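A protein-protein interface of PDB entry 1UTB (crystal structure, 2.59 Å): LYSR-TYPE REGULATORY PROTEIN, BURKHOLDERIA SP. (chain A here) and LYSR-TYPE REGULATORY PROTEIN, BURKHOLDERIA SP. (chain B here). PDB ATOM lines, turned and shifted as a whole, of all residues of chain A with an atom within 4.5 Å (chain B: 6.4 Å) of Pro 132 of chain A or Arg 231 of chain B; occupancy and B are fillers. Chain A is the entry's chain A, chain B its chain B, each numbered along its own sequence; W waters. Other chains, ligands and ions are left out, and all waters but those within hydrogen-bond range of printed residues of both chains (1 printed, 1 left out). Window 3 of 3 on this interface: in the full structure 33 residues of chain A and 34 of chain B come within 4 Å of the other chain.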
ATOM      1  N   PHE A 101      16.622   4.796   3.353  1.00  0.00           N
ATOM      2  CA  PHE A 101      16.358   5.128   1.932  1.00  0.00           C
ATOM      3  C   PHE A 101      16.174   6.633   1.702  1.00  0.00           C
ATOM      4  O   PHE A 101      16.288   7.119   0.564  1.00  0.00           O
ATOM      5  CB  PHE A 101      15.159   4.340   1.365  1.00  0.00           C
ATOM      6  N   MET A 124      30.063   0.514  -0.538  1.00  0.00           N
ATOM      7  CA  MET A 124      29.456   1.493  -1.444  1.00  0.00           C
ATOM      8  C   MET A 124      28.459   0.836  -2.410  1.00  0.00           C
ATOM      9  O   MET A 124      27.463   1.452  -2.806  1.00  0.00           O
ATOM     10  CB  MET A 124      30.542   2.228  -2.254  1.00  0.00           C
ATOM     11  CG  MET A 124      31.463   3.131  -1.433  1.00  0.00           C
ATOM     12  SD  MET A 124      30.678   4.162  -0.198  1.00  0.00           S
ATOM     13  CE  MET A 124      29.517   5.020  -1.240  1.00  0.00           C
ATOM     14  N   LEU A 127      25.292   0.267  -0.346  1.00  0.00           N
ATOM     15  CA  LEU A 127      24.601   1.542  -0.123  1.00  0.00           C
ATOM     16  C   LEU A 127      23.896   2.079  -1.375  1.00  0.00           C
ATOM     17  O   LEU A 127      22.910   2.795  -1.257  1.00  0.00           O
ATOM     18  CB  LEU A 127      25.561   2.607   0.409  1.00  0.00           C
ATOM     19  CG  LEU A 127      26.203   2.281   1.752  1.00  0.00           C
ATOM     20  CD1 LEU A 127      27.297   3.275   2.078  1.00  0.00           C
ATOM     21  CD2 LEU A 127      25.157   2.263   2.848  1.00  0.00           C
ATOM     22  N   ALA A 128      24.373   1.728  -2.564  1.00  0.00           N
ATOM     23  CA  ALA A 128      23.780   2.255  -3.795  1.00  0.00           C
ATOM     24  C   ALA A 128      22.277   2.016  -3.783  1.00  0.00           C
ATOM     25  O   ALA A 128      21.493   2.868  -4.193  1.00  0.00           O
ATOM     26  CB  ALA A 128      24.404   1.609  -5.016  1.00  0.00           C
ATOM     27  N   ARG A 130      20.624   0.631  -0.791  1.00  0.00           N
ATOM     28  CA  ARG A 130      20.039   0.660   0.556  1.00  0.00           C
ATOM     29  C   ARG A 130      19.932   2.035   1.190  1.00  0.00           C
ATOM     30  O   ARG A 130      19.135   2.240   2.105  1.00  0.00           O
ATOM     31  CB  ARG A 130      20.847  -0.247   1.485  1.00  0.00           C
ATOM     32  CG  ARG A 130      20.618  -1.715   1.176  1.00  0.00           C
ATOM     33  CD  ARG A 130      21.797  -2.602   1.391  1.00  0.00           C
ATOM     34  NE  ARG A 130      21.614  -3.331   2.628  1.00  0.00           N
ATOM     35  CZ  ARG A 130      21.927  -4.598   2.824  1.00  0.00           C
ATOM     36  NH1 ARG A 130      22.461  -5.342   1.859  1.00  0.00           N
ATOM     37  NH2 ARG A 130      21.705  -5.121   4.014  1.00  0.00           N
ATOM     38  N   ALA A 131      20.760   2.965   0.731  1.00  0.00           N
ATOM     39  CA  ALA A 131      20.800   4.319   1.273  1.00  0.00           C
ATOM     40  C   ALA A 131      21.401   5.234   0.207  1.00  0.00           C
ATOM     41  O   ALA A 131      22.532   5.679   0.352  1.00  0.00           O
ATOM     42  CB  ALA A 131      21.624   4.346   2.562  1.00  0.00           C
ATOM     43  N   PRO A 132      20.648   5.495  -0.865  1.00  0.00           N
ATOM     44  CA  PRO A 132      21.176   6.198  -2.045  1.00  0.00           C
ATOM     45  C   PRO A 132      21.625   7.638  -1.814  1.00  0.00           C
ATOM     46  O   PRO A 132      22.369   8.155  -2.643  1.00  0.00           O
ATOM     47  CB  PRO A 132      19.993   6.184  -3.034  1.00  0.00           C
ATOM     48  CG  PRO A 132      19.061   5.124  -2.527  1.00  0.00           C
ATOM     49  CD  PRO A 132      19.231   5.135  -1.041  1.00  0.00           C
ATOM     50  N   HIS A 133      21.212   8.252  -0.711  1.00  0.00           N
ATOM     51  CA  HIS A 133      21.443   9.681  -0.478  1.00  0.00           C
ATOM     52  C   HIS A 133      22.385   9.997   0.688  1.00  0.00           C
ATOM     53  O   HIS A 133      22.629  11.170   0.972  1.00  0.00           O
ATOM     54  CB  HIS A 133      20.088  10.395  -0.286  1.00  0.00           C
ATOM     55  CG  HIS A 133      19.097  10.087  -1.365  1.00  0.00           C
ATOM     56  ND1 HIS A 133      17.807   9.682  -1.100  1.00  0.00           N
ATOM     57  CD2 HIS A 133      19.226  10.073  -2.715  1.00  0.00           C
ATOM     58  CE1 HIS A 133      17.177   9.448  -2.241  1.00  0.00           C
ATOM     59  NE2 HIS A 133      18.016   9.680  -3.236  1.00  0.00           N
ATOM     60  N   ILE A 134      22.915   8.985   1.374  1.00  0.00           N
ATOM     61  CA  ILE A 134      23.901   9.272   2.419  1.00  0.00           C
ATOM     62  C   ILE A 134      25.263   9.561   1.794  1.00  0.00           C
ATOM     63  O   ILE A 134      25.486   9.372   0.602  1.00  0.00           O
ATOM     64  CB  ILE A 134      24.009   8.144   3.508  1.00  0.00           C
ATOM     65  CG1 ILE A 134      24.583   6.845   2.938  1.00  0.00           C
ATOM     66  CG2 ILE A 134      22.664   7.892   4.156  1.00  0.00           C
ATOM     67  CD1 ILE A 134      25.054   5.916   4.009  1.00  0.00           C
ATOM     68  N   GLN A 135      26.158  10.040   2.631  1.00  0.00           N
ATOM     69  CA  GLN A 135      27.484  10.417   2.230  1.00  0.00           C
ATOM     70  C   GLN A 135      28.420   9.769   3.222  1.00  0.00           C
ATOM     71  O   GLN A 135      28.189   9.791   4.447  1.00  0.00           O
ATOM     72  CB  GLN A 135      27.638  11.932   2.279  1.00  0.00           C
ATOM     73  CG  GLN A 135      26.959  12.668   1.118  1.00  0.00           C
ATOM     74  CD  GLN A 135      27.281  14.160   1.128  1.00  0.00           C
ATOM     75  OE1 GLN A 135      28.162  14.622   0.387  1.00  0.00           O
ATOM     76  NE2 GLN A 135      26.589  14.908   1.985  1.00  0.00           N
ATOM     77  N   ILE A 136      29.474   9.167   2.681  1.00  0.00           N
ATOM     78  CA  ILE A 136      30.478   8.504   3.494  1.00  0.00           C
ATOM     79  C   ILE A 136      31.741   9.296   3.351  1.00  0.00           C
ATOM     80  O   ILE A 136      31.975   9.906   2.322  1.00  0.00           O
ATOM     81  CB  ILE A 136      30.688   7.065   3.001  1.00  0.00           C
ATOM     82  CG1 ILE A 136      29.362   6.283   3.043  1.00  0.00           C
ATOM     83  CG2 ILE A 136      31.763   6.394   3.810  1.00  0.00           C
ATOM     84  CD1 ILE A 136      28.847   5.965   4.444  1.00  0.00           C
ATOM     85  N   GLU B 203      27.537  10.728  -9.618  1.00  0.00           N
ATOM     86  CA  GLU B 203      28.083  10.706  -8.261  1.00  0.00           C
ATOM     87  C   GLU B 203      29.603  10.497  -8.297  1.00  0.00           C
ATOM     88  O   GLU B 203      30.130   9.939  -9.249  1.00  0.00           O
ATOM     89  CB  GLU B 203      27.427   9.592  -7.456  1.00  0.00           C
ATOM     90  CG  GLU B 203      25.947   9.809  -7.163  1.00  0.00           C
ATOM     91  CD  GLU B 203      25.303   8.590  -6.519  1.00  0.00           C
ATOM     92  OE1 GLU B 203      25.259   7.522  -7.196  1.00  0.00           O
ATOM     93  OE2 GLU B 203      24.873   8.686  -5.335  1.00  0.00           O
ATOM     94  N   HIS B 204      30.295  10.939  -7.252  1.00  0.00           N
ATOM     95  CA  HIS B 204      31.756  10.989  -7.245  1.00  0.00           C
ATOM     96  C   HIS B 204      32.370  10.438  -5.973  1.00  0.00           C
ATOM     97  O   HIS B 204      31.780  10.540  -4.888  1.00  0.00           O
ATOM     98  CB  HIS B 204      32.271  12.428  -7.356  1.00  0.00           C
ATOM     99  CG  HIS B 204      31.770  13.168  -8.545  1.00  0.00           C
ATOM    100  ND1 HIS B 204      32.610  13.647  -9.523  1.00  0.00           N
ATOM    101  CD2 HIS B 204      30.522  13.538  -8.904  1.00  0.00           C
ATOM    102  CE1 HIS B 204      31.899  14.269 -10.446  1.00  0.00           C
ATOM    103  NE2 HIS B 204      30.628  14.220 -10.091  1.00  0.00           N
ATOM    104  N   VAL B 205      33.578   9.885  -6.131  1.00  0.00           N
ATOM    105  CA  VAL B 205      34.482   9.642  -5.021  1.00  0.00           C
ATOM    106  C   VAL B 205      35.554  10.715  -5.125  1.00  0.00           C
ATOM    107  O   VAL B 205      36.101  10.962  -6.212  1.00  0.00           O
ATOM    108  CB  VAL B 205      35.100   8.210  -5.022  1.00  0.00           C
ATOM    109  CG1 VAL B 205      35.752   7.860  -6.348  1.00  0.00           C
ATOM    110  CG2 VAL B 205      36.121   8.066  -3.894  1.00  0.00           C
ATOM    111  N   ARG B 228      29.171  18.981  -7.385  1.00  0.00           N
ATOM    112  CA  ARG B 228      29.537  17.573  -7.346  1.00  0.00           C
ATOM    113  C   ARG B 228      28.834  16.861  -6.199  1.00  0.00           C
ATOM    114  O   ARG B 228      29.014  17.190  -5.027  1.00  0.00           O
ATOM    115  CB  ARG B 228      31.046  17.446  -7.195  1.00  0.00           C
ATOM    116  CG  ARG B 228      31.730  16.661  -8.314  1.00  0.00           C
ATOM    117  CD  ARG B 228      33.179  17.056  -8.563  1.00  0.00           C
ATOM    118  NE  ARG B 228      33.839  17.434  -7.314  1.00  0.00           N
ATOM    119  CZ  ARG B 228      34.915  16.848  -6.803  1.00  0.00           C
ATOM    120  NH1 ARG B 228      35.527  15.835  -7.417  1.00  0.00           N
ATOM    121  NH2 ARG B 228      35.399  17.298  -5.658  1.00  0.00           N
ATOM    122  N   ARG B 229      28.031  15.872  -6.569  1.00  0.00           N
ATOM    123  CA  ARG B 229      27.427  14.937  -5.616  1.00  0.00           C
ATOM    124  C   ARG B 229      28.520  14.033  -5.008  1.00  0.00           C
ATOM    125  O   ARG B 229      28.893  13.023  -5.592  1.00  0.00           O
ATOM    126  CB  ARG B 229      26.348  14.095  -6.325  1.00  0.00           C
ATOM    127  CG  ARG B 229      25.250  14.916  -7.031  1.00  0.00           C
ATOM    128  CD  ARG B 229      24.286  14.087  -7.862  1.00  0.00           C
ATOM    129  NE  ARG B 229      23.595  13.125  -7.007  1.00  0.00           N
ATOM    130  CZ  ARG B 229      23.016  11.999  -7.419  1.00  0.00           C
ATOM    131  NH1 ARG B 229      23.009  11.665  -8.704  1.00  0.00           N
ATOM    132  NH2 ARG B 229      22.433  11.199  -6.520  1.00  0.00           N
ATOM    133  N   MET B 230      29.055  14.422  -3.859  1.00  0.00           N
ATOM    134  CA  MET B 230      30.170  13.705  -3.262  1.00  0.00           C
ATOM    135  C   MET B 230      29.681  12.557  -2.394  1.00  0.00           C
ATOM    136  O   MET B 230      29.560  12.693  -1.173  1.00  0.00           O
ATOM    137  CB  MET B 230      31.041  14.656  -2.446  1.00  0.00           C
ATOM    138  CG  MET B 230      31.647  15.804  -3.266  1.00  0.00           C
ATOM    139  SD  MET B 230      32.683  15.312  -4.700  1.00  0.00           S
ATOM    140  CE  MET B 230      33.969  14.457  -3.825  1.00  0.00           C
ATOM    141  N   ARG B 231      29.399  11.431  -3.054  1.00  0.00           N
ATOM    142  CA  ARG B 231      29.021  10.165  -2.401  1.00  0.00           C
ATOM    143  C   ARG B 231      30.026   9.659  -1.355  1.00  0.00           C
ATOM    144  O   ARG B 231      29.657   9.168  -0.283  1.00  0.00           O
ATOM    145  CB  ARG B 231      28.881   9.079  -3.457  1.00  0.00           C
ATOM    146  CG  ARG B 231      27.517   8.538  -3.564  1.00  0.00           C
ATOM    147  CD  ARG B 231      27.065   7.844  -2.306  1.00  0.00           C
ATOM    148  NE  ARG B 231      26.159   6.727  -2.586  1.00  0.00           N
ATOM    149  CZ  ARG B 231      25.340   6.192  -1.688  1.00  0.00           C
ATOM    150  NH1 ARG B 231      25.302   6.660  -0.442  1.00  0.00           N
ATOM    151  NH2 ARG B 231      24.560   5.181  -2.031  1.00  0.00           N
ATOM    152  N   LEU B 232      31.303   9.772  -1.699  1.00  0.00           N
ATOM    153  CA  LEU B 232      32.374   9.238  -0.882  1.00  0.00           C
ATOM    154  C   LEU B 232      33.614  10.117  -1.021  1.00  0.00           C
ATOM    155  O   LEU B 232      33.948  10.581  -2.105  1.00  0.00           O
ATOM    156  CB  LEU B 232      32.683   7.786  -1.287  1.00  0.00           C
ATOM    157  CG  LEU B 232      34.001   7.175  -0.804  1.00  0.00           C
ATOM    158  CD1 LEU B 232      33.946   6.830   0.665  1.00  0.00           C
ATOM    159  CD2 LEU B 232      34.345   5.962  -1.630  1.00  0.00           C
ATOM    160  N   VAL B 233      34.273  10.329   0.107  1.00  0.00           N
ATOM    161  CA  VAL B 233      35.521  11.044   0.162  1.00  0.00           C
ATOM    162  C   VAL B 233      36.478  10.152   0.928  1.00  0.00           C
ATOM    163  O   VAL B 233      36.116   9.599   1.965  1.00  0.00           O
ATOM    164  CB  VAL B 233      35.374  12.414   0.923  1.00  0.00           C
ATOM    165  CG1 VAL B 233      36.730  13.069   1.153  1.00  0.00           C
ATOM    166  CG2 VAL B 233      34.476  13.336   0.150  1.00  0.00           C
ATOM    167  N   LEU B 249      30.409   5.227  -9.291  1.00  0.00           N
ATOM    168  CA  LEU B 249      31.104   6.473  -8.958  1.00  0.00           C
ATOM    169  C   LEU B 249      32.127   6.840 -10.027  1.00  0.00           C
ATOM    170  O   LEU B 249      32.672   5.974 -10.718  1.00  0.00           O
ATOM    171  CB  LEU B 249      31.822   6.359  -7.610  1.00  0.00           C
ATOM    172  CG  LEU B 249      30.927   6.037  -6.417  1.00  0.00           C
ATOM    173  CD1 LEU B 249      31.741   5.753  -5.151  1.00  0.00           C
ATOM    174  CD2 LEU B 249      29.954   7.170  -6.173  1.00  0.00           C
HETATM  175  O   HOH W   1      28.025  16.689  -1.746  1.00  0.00           O
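NH2 of Arg 229 of chain B is in salt-bridge range of OE2 of Glu 203 of chain B (3.7 Å).
OE2 of Glu 203 of chain B lies within salt-bridge range of NE of Arg 231 of chain B, 3.6 Å away.
O of His 204 of chain B is in hydrogen-bond range of N of Arg 231 of chain B (3.1 Å).
The backbone carbonyl oxygen (O) of His 204 of chain B is in hydrogen-bond range of the backbone NH (N) of Leu 232 of chain B.
NH2 of Arg 228 of chain B lies close to SD of Met 230 of chain B (3.5 Å).
The guanidinium group of Arg 231 of chain B sits at hydrogen-bond distance from the backbone carbonyl oxygen of Leu 127 of chain A (3.0 Å).
The guanidinium group (NH1) of Arg 231 of chain B is in hydrogen-bond range of the backbone carbonyl oxygen (O) of Ala 131 of chain A, at 3.0 Å.
O of Ile 134 of chain A sits at hydrogen-bond distance from NH1 of Arg 231 of chain B, 2.9 Å away.
The side-chain amide oxygen (OE1) of Gln 135 of chain A lies close to the backbone carbonyl oxygen (O) of Met 230 of chain B (2.8 Å).
N of Ile 136 of chain A is in hydrogen-bond range of O of Arg 231 of chain B, at 3.0 Å.
The backbone carbonyl oxygen (O) of Ile 136 of chain A sits at hydrogen-bond distance from the backbone NH (N) of Val 233 of chain B (3.2 Å).
The guanidinium group of Arg 231 of chain B sits close to the backbone NH of Ala 128 of chain A, at 3.5 Å.
Water W1 lies within hydrogen-bond range of the side-chain amide oxygen of Gln 135 of chain A, the backbone NH of Met 230 of chain B and the backbone carbonyl oxygen of Arg 228 of chain B.
Met 124 of chain A touches Arg 231 of chain B (CE to CD, 3.9 Å).
Glu 203 of chain B touches Pro 132 of chain A (OE2 to O, 3.7 Å).
Pro 132 of chain A touches Arg 231 of chain B.
O of Arg 231 of chain B touches CA of Gln 135 of chain A, 3.5 Å away.
Leu 232 of chain B touches Ile 136 of chain A.
Of the 11 printed residues of chain A, 8 touch a printed residue of chain B.
Hydrophobic or aromatic side chains of chain A that line the printed part of chain B: Met 124, Leu 127, Ile 134 and Ile 136.
Hydrophobic or aromatic side chains of chain B that line the printed part of chain A: Leu 232.
Of the printed residues of chain B, Leu 127 of chain A touches Arg 231 (3.0 Å).
Of the printed residues of chain B, Ala 128 of chain A touches Arg 231.
Printed residues of chain B within 4 Å of Ala 131 of chain A: Arg 231 (3.0 Å).
Of chain B, only Glu 203 (3.7 Å) and Arg 231 (3.5 Å) come within 4 Å of Pro 132 of chain A.
Of the printed residues of chain B, Gln 135 of chain A touches Met 230 and Arg 231.
Printed residues of chain A within 4 Å of Glu 203 of chain B: Pro 132.
Val 205 of chain B touches none of the printed residues of chain A.
Of chain A, only Met 124, Leu 127, Ala 128, Ala 131, Pro 132, Ile 134, Gln 135 and Ile 136 come within 4 Å of Arg 231 of chain B.
Leu 249 of chain B touches none of the printed residues of chain A.
The nearest residue of chain B that does not touch Pro 132 of chain A is Arg 229 of chain B (4.9 Å).
The nearest residue of chain A that does not touch Arg 231 of chain B is His 133 of chain A (4.4 Å).
The nearest printed residue of chain A that does not touch Val 233 of chain B is Gln 135 of chain A (6.4 Å).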
